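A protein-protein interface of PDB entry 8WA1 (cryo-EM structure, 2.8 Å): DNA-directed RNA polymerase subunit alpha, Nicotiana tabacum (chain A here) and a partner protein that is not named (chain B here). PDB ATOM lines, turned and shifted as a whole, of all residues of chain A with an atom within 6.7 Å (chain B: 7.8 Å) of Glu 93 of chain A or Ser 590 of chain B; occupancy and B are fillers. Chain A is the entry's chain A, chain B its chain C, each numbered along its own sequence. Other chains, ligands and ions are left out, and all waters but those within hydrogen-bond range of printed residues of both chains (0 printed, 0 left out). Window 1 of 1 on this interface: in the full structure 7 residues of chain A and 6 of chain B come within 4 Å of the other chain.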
ATOM      1  N   ARG A  26       1.120  -1.254 -13.627  1.00  0.00           N
ATOM      2  CA  ARG A  26       1.963  -0.103 -13.920  1.00  0.00           C
ATOM      3  C   ARG A  26       1.159   1.125 -14.327  1.00  0.00           C
ATOM      4  O   ARG A  26       1.745   2.122 -14.760  1.00  0.00           O
ATOM      5  CB  ARG A  26       2.974  -0.456 -15.013  1.00  0.00           C
ATOM      6  CG  ARG A  26       3.942  -1.555 -14.619  1.00  0.00           C
ATOM      7  CD  ARG A  26       4.879  -1.913 -15.758  1.00  0.00           C
ATOM      8  NE  ARG A  26       4.188  -2.630 -16.825  1.00  0.00           N
ATOM      9  CZ  ARG A  26       4.792  -3.146 -17.889  1.00  0.00           C
ATOM     10  NH1 ARG A  26       4.084  -3.783 -18.810  1.00  0.00           N
ATOM     11  NH2 ARG A  26       6.105  -3.027 -18.031  1.00  0.00           N
ATOM     12  N   LEU A  88      19.418  -1.953 -21.954  1.00  0.00           N
ATOM     13  CA  LEU A  88      19.395  -0.662 -21.272  1.00  0.00           C
ATOM     14  C   LEU A  88      18.022  -0.009 -21.377  1.00  0.00           C
ATOM     15  O   LEU A  88      17.517   0.558 -20.400  1.00  0.00           O
ATOM     16  CB  LEU A  88      20.472   0.261 -21.842  1.00  0.00           C
ATOM     17  CG  LEU A  88      21.919  -0.111 -21.519  1.00  0.00           C
ATOM     18  CD1 LEU A  88      22.879   0.948 -22.039  1.00  0.00           C
ATOM     19  CD2 LEU A  88      22.095  -0.318 -20.025  1.00  0.00           C
ATOM     20  N   MET A  89      17.404  -0.077 -22.558  1.00  0.00           N
ATOM     21  CA  MET A  89      16.061   0.471 -22.719  1.00  0.00           C
ATOM     22  C   MET A  89      15.043  -0.315 -21.903  1.00  0.00           C
ATOM     23  O   MET A  89      14.031   0.240 -21.460  1.00  0.00           O
ATOM     24  CB  MET A  89      15.673   0.489 -24.197  1.00  0.00           C
ATOM     25  CG  MET A  89      16.477   1.469 -25.035  1.00  0.00           C
ATOM     26  SD  MET A  89      16.298   3.166 -24.453  1.00  0.00           S
ATOM     27  CE  MET A  89      17.410   4.034 -25.559  1.00  0.00           C
ATOM     28  N   ASN A  90      15.286  -1.611 -21.704  1.00  0.00           N
ATOM     29  CA  ASN A  90      14.415  -2.394 -20.832  1.00  0.00           C
ATOM     30  C   ASN A  90      14.619  -2.021 -19.368  1.00  0.00           C
ATOM     31  O   ASN A  90      13.662  -2.003 -18.585  1.00  0.00           O
ATOM     32  CB  ASN A  90      14.664  -3.888 -21.048  1.00  0.00           C
ATOM     33  CG  ASN A  90      14.227  -4.359 -22.422  1.00  0.00           C
ATOM     34  OD1 ASN A  90      13.940  -3.551 -23.305  1.00  0.00           O
ATOM     35  ND2 ASN A  90      14.176  -5.672 -22.607  1.00  0.00           N
ATOM     36  N   LEU A  91      15.862  -1.723 -18.981  1.00  0.00           N
ATOM     37  CA  LEU A  91      16.141  -1.344 -17.599  1.00  0.00           C
ATOM     38  C   LEU A  91      15.571   0.030 -17.271  1.00  0.00           C
ATOM     39  O   LEU A  91      15.100   0.262 -16.152  1.00  0.00           O
ATOM     40  CB  LEU A  91      17.647  -1.371 -17.340  1.00  0.00           C
ATOM     41  CG  LEU A  91      18.307  -2.744 -17.201  1.00  0.00           C
ATOM     42  CD1 LEU A  91      19.815  -2.602 -17.058  1.00  0.00           C
ATOM     43  CD2 LEU A  91      17.725  -3.496 -16.018  1.00  0.00           C
ATOM     44  N   LYS A  92      15.606   0.958 -18.231  1.00  0.00           N
ATOM     45  CA  LYS A  92      15.096   2.299 -17.969  1.00  0.00           C
ATOM     46  C   LYS A  92      13.582   2.330 -17.805  1.00  0.00           C
ATOM     47  O   LYS A  92      13.052   3.335 -17.319  1.00  0.00           O
ATOM     48  CB  LYS A  92      15.509   3.261 -19.084  1.00  0.00           C
ATOM     49  CG  LYS A  92      14.697   3.127 -20.358  1.00  0.00           C
ATOM     50  CD  LYS A  92      14.963   4.282 -21.308  1.00  0.00           C
ATOM     51  CE  LYS A  92      14.569   5.611 -20.684  1.00  0.00           C
ATOM     52  NZ  LYS A  92      13.133   5.636 -20.288  1.00  0.00           N
ATOM     53  N   GLU A  93      12.880   1.267 -18.192  1.00  0.00           N
ATOM     54  CA  GLU A  93      11.435   1.187 -18.040  1.00  0.00           C
ATOM     55  C   GLU A  93      11.010   0.504 -16.747  1.00  0.00           C
ATOM     56  O   GLU A  93       9.807   0.362 -16.505  1.00  0.00           O
ATOM     57  CB  GLU A  93      10.818   0.448 -19.233  1.00  0.00           C
ATOM     58  CG  GLU A  93      11.066   1.114 -20.578  1.00  0.00           C
ATOM     59  CD  GLU A  93      10.352   2.445 -20.717  1.00  0.00           C
ATOM     60  OE1 GLU A  93       9.333   2.653 -20.026  1.00  0.00           O
ATOM     61  OE2 GLU A  93      10.809   3.283 -21.522  1.00  0.00           O
ATOM     62  N   ILE A  94      11.956   0.080 -15.916  1.00  0.00           N
ATOM     63  CA  ILE A  94      11.632  -0.582 -14.658  1.00  0.00           C
ATOM     64  C   ILE A  94      11.225   0.466 -13.632  1.00  0.00           C
ATOM     65  O   ILE A  94      11.949   1.442 -13.400  1.00  0.00           O
ATOM     66  CB  ILE A  94      12.820  -1.416 -14.158  1.00  0.00           C
ATOM     67  CG1 ILE A  94      13.116  -2.559 -15.133  1.00  0.00           C
ATOM     68  CG2 ILE A  94      12.547  -1.956 -12.764  1.00  0.00           C
ATOM     69  CD1 ILE A  94      14.235  -3.468 -14.679  1.00  0.00           C
ATOM     70  N   ILE A  95      10.065   0.267 -13.012  1.00  0.00           N
ATOM     71  CA  ILE A  95       9.545   1.174 -11.995  1.00  0.00           C
ATOM     72  C   ILE A  95       9.949   0.654 -10.623  1.00  0.00           C
ATOM     73  O   ILE A  95       9.869  -0.551 -10.356  1.00  0.00           O
ATOM     74  CB  ILE A  95       8.018   1.318 -12.100  1.00  0.00           C
ATOM     75  CG1 ILE A  95       7.363  -0.053 -12.272  1.00  0.00           C
ATOM     76  CG2 ILE A  95       7.650   2.243 -13.247  1.00  0.00           C
ATOM     77  CD1 ILE A  95       5.869  -0.035 -12.072  1.00  0.00           C
ATOM     78  N   GLN A 134       8.114  -7.457 -15.353  1.00  0.00           N
ATOM     79  CA  GLN A 134       8.880  -6.694 -16.330  1.00  0.00           C
ATOM     80  C   GLN A 134      10.042  -7.519 -16.870  1.00  0.00           C
ATOM     81  O   GLN A 134      10.721  -8.231 -16.125  1.00  0.00           O
ATOM     82  CB  GLN A 134       9.394  -5.397 -15.706  1.00  0.00           C
ATOM     83  CG  GLN A 134       8.291  -4.475 -15.213  1.00  0.00           C
ATOM     84  CD  GLN A 134       8.801  -3.094 -14.853  1.00  0.00           C
ATOM     85  OE1 GLN A 134       9.110  -2.815 -13.695  1.00  0.00           O
ATOM     86  NE2 GLN A 134       8.886  -2.218 -15.848  1.00  0.00           N
ATOM     87  N   ARG A 180       2.189   9.921 -14.675  1.00  0.00           N
ATOM     88  CA  ARG A 180       2.242   9.845 -16.130  1.00  0.00           C
ATOM     89  C   ARG A 180       1.572  11.048 -16.785  1.00  0.00           C
ATOM     90  O   ARG A 180       2.121  11.629 -17.727  1.00  0.00           O
ATOM     91  CB  ARG A 180       1.591   8.549 -16.612  1.00  0.00           C
ATOM     92  CG  ARG A 180       2.403   7.302 -16.320  1.00  0.00           C
ATOM     93  CD  ARG A 180       1.682   6.061 -16.812  1.00  0.00           C
ATOM     94  NE  ARG A 180       2.550   4.888 -16.810  1.00  0.00           N
ATOM     95  CZ  ARG A 180       3.287   4.507 -17.848  1.00  0.00           C
ATOM     96  NH1 ARG A 180       3.259   5.205 -18.975  1.00  0.00           N
ATOM     97  NH2 ARG A 180       4.050   3.426 -17.760  1.00  0.00           N
ATOM     98  N   PRO B 587      17.789  12.465 -28.572  1.00  0.00           N
ATOM     99  CA  PRO B 587      16.830  11.771 -27.702  1.00  0.00           C
ATOM    100  C   PRO B 587      16.263  10.520 -28.356  1.00  0.00           C
ATOM    101  O   PRO B 587      15.965  10.498 -29.552  1.00  0.00           O
ATOM    102  CB  PRO B 587      15.735  12.819 -27.468  1.00  0.00           C
ATOM    103  CG  PRO B 587      16.354  14.122 -27.830  1.00  0.00           C
ATOM    104  CD  PRO B 587      17.298  13.805 -28.938  1.00  0.00           C
ATOM    105  N   PHE B 588      16.118   9.473 -27.549  1.00  0.00           N
ATOM    106  CA  PHE B 588      15.497   8.221 -27.965  1.00  0.00           C
ATOM    107  C   PHE B 588      14.319   7.937 -27.045  1.00  0.00           C
ATOM    108  O   PHE B 588      14.495   7.815 -25.828  1.00  0.00           O
ATOM    109  CB  PHE B 588      16.498   7.064 -27.926  1.00  0.00           C
ATOM    110  CG  PHE B 588      17.350   6.956 -29.157  1.00  0.00           C
ATOM    111  CD1 PHE B 588      18.458   7.769 -29.326  1.00  0.00           C
ATOM    112  CD2 PHE B 588      17.049   6.030 -30.142  1.00  0.00           C
ATOM    113  CE1 PHE B 588      19.245   7.666 -30.457  1.00  0.00           C
ATOM    114  CE2 PHE B 588      17.832   5.921 -31.275  1.00  0.00           C
ATOM    115  CZ  PHE B 588      18.931   6.741 -31.434  1.00  0.00           C
ATOM    116  N   PHE B 589      13.127   7.828 -27.624  1.00  0.00           N
ATOM    117  CA  PHE B 589      11.909   7.572 -26.866  1.00  0.00           C
ATOM    118  C   PHE B 589      11.298   6.259 -27.325  1.00  0.00           C
ATOM    119  O   PHE B 589      11.160   6.022 -28.529  1.00  0.00           O
ATOM    120  CB  PHE B 589      10.897   8.709 -27.033  1.00  0.00           C
ATOM    121  CG  PHE B 589      11.358  10.019 -26.465  1.00  0.00           C
ATOM    122  CD1 PHE B 589      11.254  10.275 -25.107  1.00  0.00           C
ATOM    123  CD2 PHE B 589      11.886  10.997 -27.288  1.00  0.00           C
ATOM    124  CE1 PHE B 589      11.675  11.481 -24.583  1.00  0.00           C
ATOM    125  CE2 PHE B 589      12.308  12.205 -26.769  1.00  0.00           C
ATOM    126  CZ  PHE B 589      12.203  12.447 -25.415  1.00  0.00           C
ATOM    127  N   SER B 590      10.938   5.407 -26.363  1.00  0.00           N
ATOM    128  CA  SER B 590      10.315   4.133 -26.701  1.00  0.00           C
ATOM    129  C   SER B 590       8.842   4.310 -27.049  1.00  0.00           C
ATOM    130  O   SER B 590       8.314   3.604 -27.916  1.00  0.00           O
ATOM    131  CB  SER B 590      10.477   3.147 -25.544  1.00  0.00           C
ATOM    132  OG  SER B 590      11.843   2.976 -25.206  1.00  0.00           O
ATOM    133  N   ASN B 591       8.165   5.246 -26.388  1.00  0.00           N
ATOM    134  CA  ASN B 591       6.743   5.467 -26.587  1.00  0.00           C
ATOM    135  C   ASN B 591       6.492   6.923 -26.952  1.00  0.00           C
ATOM    136  O   ASN B 591       7.276   7.815 -26.618  1.00  0.00           O
ATOM    137  CB  ASN B 591       5.936   5.097 -25.334  1.00  0.00           C
ATOM    138  CG  ASN B 591       6.212   3.685 -24.860  1.00  0.00           C
ATOM    139  OD1 ASN B 591       6.645   3.470 -23.728  1.00  0.00           O
ATOM    140  ND2 ASN B 591       5.964   2.711 -25.728  1.00  0.00           N
ATOM    141  N   SER B 592       5.378   7.151 -27.650  1.00  0.00           N
ATOM    142  CA  SER B 592       4.982   8.514 -27.985  1.00  0.00           C
ATOM    143  C   SER B 592       4.568   9.283 -26.738  1.00  0.00           C
ATOM    144  O   SER B 592       4.735  10.507 -26.666  1.00  0.00           O
ATOM    145  CB  SER B 592       3.843   8.492 -29.004  1.00  0.00           C
ATOM    146  OG  SER B 592       4.134   7.603 -30.069  1.00  0.00           O
ATOM    147  N   TYR B 593       4.017   8.576 -25.749  1.00  0.00           N
ATOM    148  CA  TYR B 593       3.624   9.221 -24.502  1.00  0.00           C
ATOM    149  C   TYR B 593       4.827   9.833 -23.798  1.00  0.00           C
ATOM    150  O   TYR B 593       4.736  10.931 -23.240  1.00  0.00           O
ATOM    151  CB  TYR B 593       2.925   8.210 -23.592  1.00  0.00           C
ATOM    152  CG  TYR B 593       1.973   7.286 -24.320  1.00  0.00           C
ATOM    153  CD1 TYR B 593       0.672   7.679 -24.602  1.00  0.00           C
ATOM    154  CD2 TYR B 593       2.376   6.018 -24.721  1.00  0.00           C
ATOM    155  CE1 TYR B 593      -0.200   6.838 -25.266  1.00  0.00           C
ATOM    156  CE2 TYR B 593       1.510   5.171 -25.385  1.00  0.00           C
ATOM    157  CZ  TYR B 593       0.223   5.585 -25.654  1.00  0.00           C
ATOM    158  OH  TYR B 593      -0.642   4.744 -26.316  1.00  0.00           O
ATOM    159  N   ASP B 594       5.970   9.142 -23.829  1.00  0.00           N
ATOM    160  CA  ASP B 594       7.173   9.672 -23.198  1.00  0.00           C
ATOM    161  C   ASP B 594       7.644  10.944 -23.891  1.00  0.00           C
ATOM    162  O   ASP B 594       8.030  11.915 -23.229  1.00  0.00           O
ATOM    163  CB  ASP B 594       8.277   8.615 -23.207  1.00  0.00           C
ATOM    164  CG  ASP B 594       7.819   7.292 -22.627  1.00  0.00           C
ATOM    165  OD1 ASP B 594       6.958   7.304 -21.722  1.00  0.00           O
ATOM    166  OD2 ASP B 594       8.318   6.241 -23.079  1.00  0.00           O
ATOM    167  N   ALA B 595       7.612  10.961 -25.225  1.00  0.00           N
ATOM    168  CA  ALA B 595       8.031  12.151 -25.956  1.00  0.00           C
ATOM    169  C   ALA B 595       7.084  13.319 -25.707  1.00  0.00           C
ATOM    170  O   ALA B 595       7.527  14.462 -25.547  1.00  0.00           O
ATOM    171  CB  ALA B 595       8.125  11.842 -27.449  1.00  0.00           C
ATOM    172  N   TRP B 611      14.166  10.266 -31.970  1.00  0.00           N
ATOM    173  CA  TRP B 611      13.947   8.935 -32.521  1.00  0.00           C
ATOM    174  C   TRP B 611      12.817   8.258 -31.758  1.00  0.00           C
ATOM    175  O   TRP B 611      12.803   8.273 -30.523  1.00  0.00           O
ATOM    176  CB  TRP B 611      15.219   8.085 -32.449  1.00  0.00           C
ATOM    177  CG  TRP B 611      16.327   8.567 -33.339  1.00  0.00           C
ATOM    178  CD1 TRP B 611      17.287   9.483 -33.028  1.00  0.00           C
ATOM    179  CD2 TRP B 611      16.594   8.148 -34.684  1.00  0.00           C
ATOM    180  NE1 TRP B 611      18.131   9.666 -34.095  1.00  0.00           N
ATOM    181  CE2 TRP B 611      17.728   8.857 -35.125  1.00  0.00           C
ATOM    182  CE3 TRP B 611      15.982   7.245 -35.558  1.00  0.00           C
ATOM    183  CZ2 TRP B 611      18.263   8.691 -36.401  1.00  0.00           C
ATOM    184  CZ3 TRP B 611      16.515   7.081 -36.825  1.00  0.00           C
ATOM    185  CH2 TRP B 611      17.644   7.801 -37.233  1.00  0.00           C
ATOM    186  N   LEU B 612      11.874   7.670 -32.491  1.00  0.00           N
ATOM    187  CA  LEU B 612      10.733   6.980 -31.903  1.00  0.00           C
ATOM    188  C   LEU B 612      10.688   5.547 -32.409  1.00  0.00           C
ATOM    189  O   LEU B 612      10.694   5.312 -33.622  1.00  0.00           O
ATOM    190  CB  LEU B 612       9.421   7.697 -32.235  1.00  0.00           C
ATOM    191  CG  LEU B 612       8.158   7.086 -31.621  1.00  0.00           C
ATOM    192  CD1 LEU B 612       8.216   7.147 -30.103  1.00  0.00           C
ATOM    193  CD2 LEU B 612       6.909   7.778 -32.142  1.00  0.00           C
ATOM    194  N   ARG B 613      10.649   4.595 -31.481  1.00  0.00           N
ATOM    195  CA  ARG B 613      10.569   3.188 -31.849  1.00  0.00           C
ATOM    196  C   ARG B 613       9.152   2.829 -32.287  1.00  0.00           C
ATOM    197  O   ARG B 613       8.171   3.197 -31.634  1.00  0.00           O
ATOM    198  CB  ARG B 613      10.999   2.309 -30.675  1.00  0.00           C
ATOM    199  CG  ARG B 613      11.079   0.827 -30.997  1.00  0.00           C
ATOM    200  CD  ARG B 613      11.547   0.029 -29.787  1.00  0.00           C
ATOM    201  NE  ARG B 613      11.569  -1.406 -30.048  1.00  0.00           N
ATOM    202  CZ  ARG B 613      11.925  -2.321 -29.152  1.00  0.00           C
ATOM    203  NH1 ARG B 613      12.292  -1.950 -27.933  1.00  0.00           N
ATOM    204  NH2 ARG B 613      11.915  -3.608 -29.472  1.00  0.00           N
ATOM    205  N   TRP B 614       9.048   2.104 -33.399  1.00  0.00           N
ATOM    206  CA  TRP B 614       7.769   1.674 -33.946  1.00  0.00           C
ATOM    207  C   TRP B 614       7.664   0.157 -33.891  1.00  0.00           C
ATOM    208  O   TRP B 614       8.677  -0.547 -33.969  1.00  0.00           O
ATOM    209  CB  TRP B 614       7.585   2.154 -35.387  1.00  0.00           C
ATOM    210  CG  TRP B 614       6.476   3.142 -35.541  1.00  0.00           C
ATOM    211  CD1 TRP B 614       6.002   3.995 -34.588  1.00  0.00           C
ATOM    212  CD2 TRP B 614       5.686   3.371 -36.713  1.00  0.00           C
ATOM    213  NE1 TRP B 614       4.971   4.749 -35.096  1.00  0.00           N
ATOM    214  CE2 TRP B 614       4.758   4.384 -36.399  1.00  0.00           C
ATOM    215  CE3 TRP B 614       5.676   2.822 -37.997  1.00  0.00           C
ATOM    216  CZ2 TRP B 614       3.830   4.857 -37.323  1.00  0.00           C
ATOM    217  CZ3 TRP B 614       4.756   3.293 -38.912  1.00  0.00           C
ATOM    218  CH2 TRP B 614       3.845   4.300 -38.571  1.00  0.00           C
ATOM    219  N   ARG B 615       6.435  -0.342 -33.754  1.00  0.00           N
ATOM    220  CA  ARG B 615       6.186  -1.778 -33.636  1.00  0.00           C
ATOM    221  C   ARG B 615       5.767  -2.335 -34.993  1.00  0.00           C
ATOM    222  O   ARG B 615       4.609  -2.680 -35.226  1.00  0.00           O
ATOM    223  CB  ARG B 615       5.133  -2.052 -32.567  1.00  0.00           C
ATOM    224  CG  ARG B 615       5.509  -1.571 -31.176  1.00  0.00           C
ATOM    225  CD  ARG B 615       6.837  -2.160 -30.735  1.00  0.00           C
ATOM    226  NE  ARG B 615       7.102  -1.912 -29.321  1.00  0.00           N
ATOM    227  CZ  ARG B 615       7.697  -0.821 -28.851  1.00  0.00           C
ATOM    228  NH1 ARG B 615       8.090   0.134 -29.683  1.00  0.00           N
ATOM    229  NH2 ARG B 615       7.896  -0.682 -27.548  1.00  0.00           N
ATOM    230  N   ILE B 658      12.786  -0.926 -35.348  1.00  0.00           N
ATOM    231  CA  ILE B 658      12.519   0.162 -36.280  1.00  0.00           C
ATOM    232  C   ILE B 658      12.387   1.447 -35.477  1.00  0.00           C
ATOM    233  O   ILE B 658      11.587   1.515 -34.538  1.00  0.00           O
ATOM    234  CB  ILE B 658      11.247  -0.086 -37.112  1.00  0.00           C
ATOM    235  CG1 ILE B 658      11.424  -1.307 -38.015  1.00  0.00           C
ATOM    236  CG2 ILE B 658      10.905   1.145 -37.940  1.00  0.00           C
ATOM    237  CD1 ILE B 658      10.209  -1.621 -38.862  1.00  0.00           C
ATOM    238  N   TYR B 659      13.166   2.461 -35.845  1.00  0.00           N
ATOM    239  CA  TYR B 659      13.148   3.749 -35.166  1.00  0.00           C
ATOM    240  C   TYR B 659      12.870   4.848 -36.177  1.00  0.00           C
ATOM    241  O   TYR B 659      13.605   4.991 -37.160  1.00  0.00           O
ATOM    242  CB  TYR B 659      14.473   4.013 -34.441  1.00  0.00           C
ATOM    243  CG  TYR B 659      14.644   3.202 -33.179  1.00  0.00           C
ATOM    244  CD1 TYR B 659      15.128   1.902 -33.225  1.00  0.00           C
ATOM    245  CD2 TYR B 659      14.313   3.735 -31.941  1.00  0.00           C
ATOM    246  CE1 TYR B 659      15.282   1.156 -32.072  1.00  0.00           C
ATOM    247  CE2 TYR B 659      14.465   2.998 -30.782  1.00  0.00           C
ATOM    248  CZ  TYR B 659      14.949   1.709 -30.854  1.00  0.00           C
ATOM    249  OH  TYR B 659      15.099   0.971 -29.703  1.00  0.00           O
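Met 89 of chain A touches Phe 588 of chain B.
Glu 93 of chain A touches Ser 590 of chain B.
NZ of Lys 92 of chain A is in salt-bridge range of OE2 of Glu 93 of chain A.
O of Glu 93 of chain A lies within hydrogen-bond range of NE2 of Gln 134 of chain A (2.8 Å).
Of the 16 printed residues of chain B, 2 touch a printed residue of chain A.
Hydrophobic or aromatic side chains of chain B that line the printed part of chain A: Phe 588.
Hydrophobic or aromatic side chains of chain A that line the printed part of chain B: Met 89.
Among the printed residues, no Asp or Glu carboxylate lies within 4 Å of a Lys or Arg side-chain nitrogen of the other chain.
Of the printed residues of chain B, Met 89 of chain A touches Phe 588 (3.95 Å).
Glu 93 of chain A touches just one residue of chain B: Ser 590.
Of the printed residues of chain A, Phe 588 of chain B touches Met 89 (3.95 Å).
The nearest residue of chain B that does not touch Glu 93 of chain A is Asp 594 of chain B (4.2 Å).
The nearest residue of chain A that does not touch Ser 590 of chain B is Met 89 of chain A (4.5 Å).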
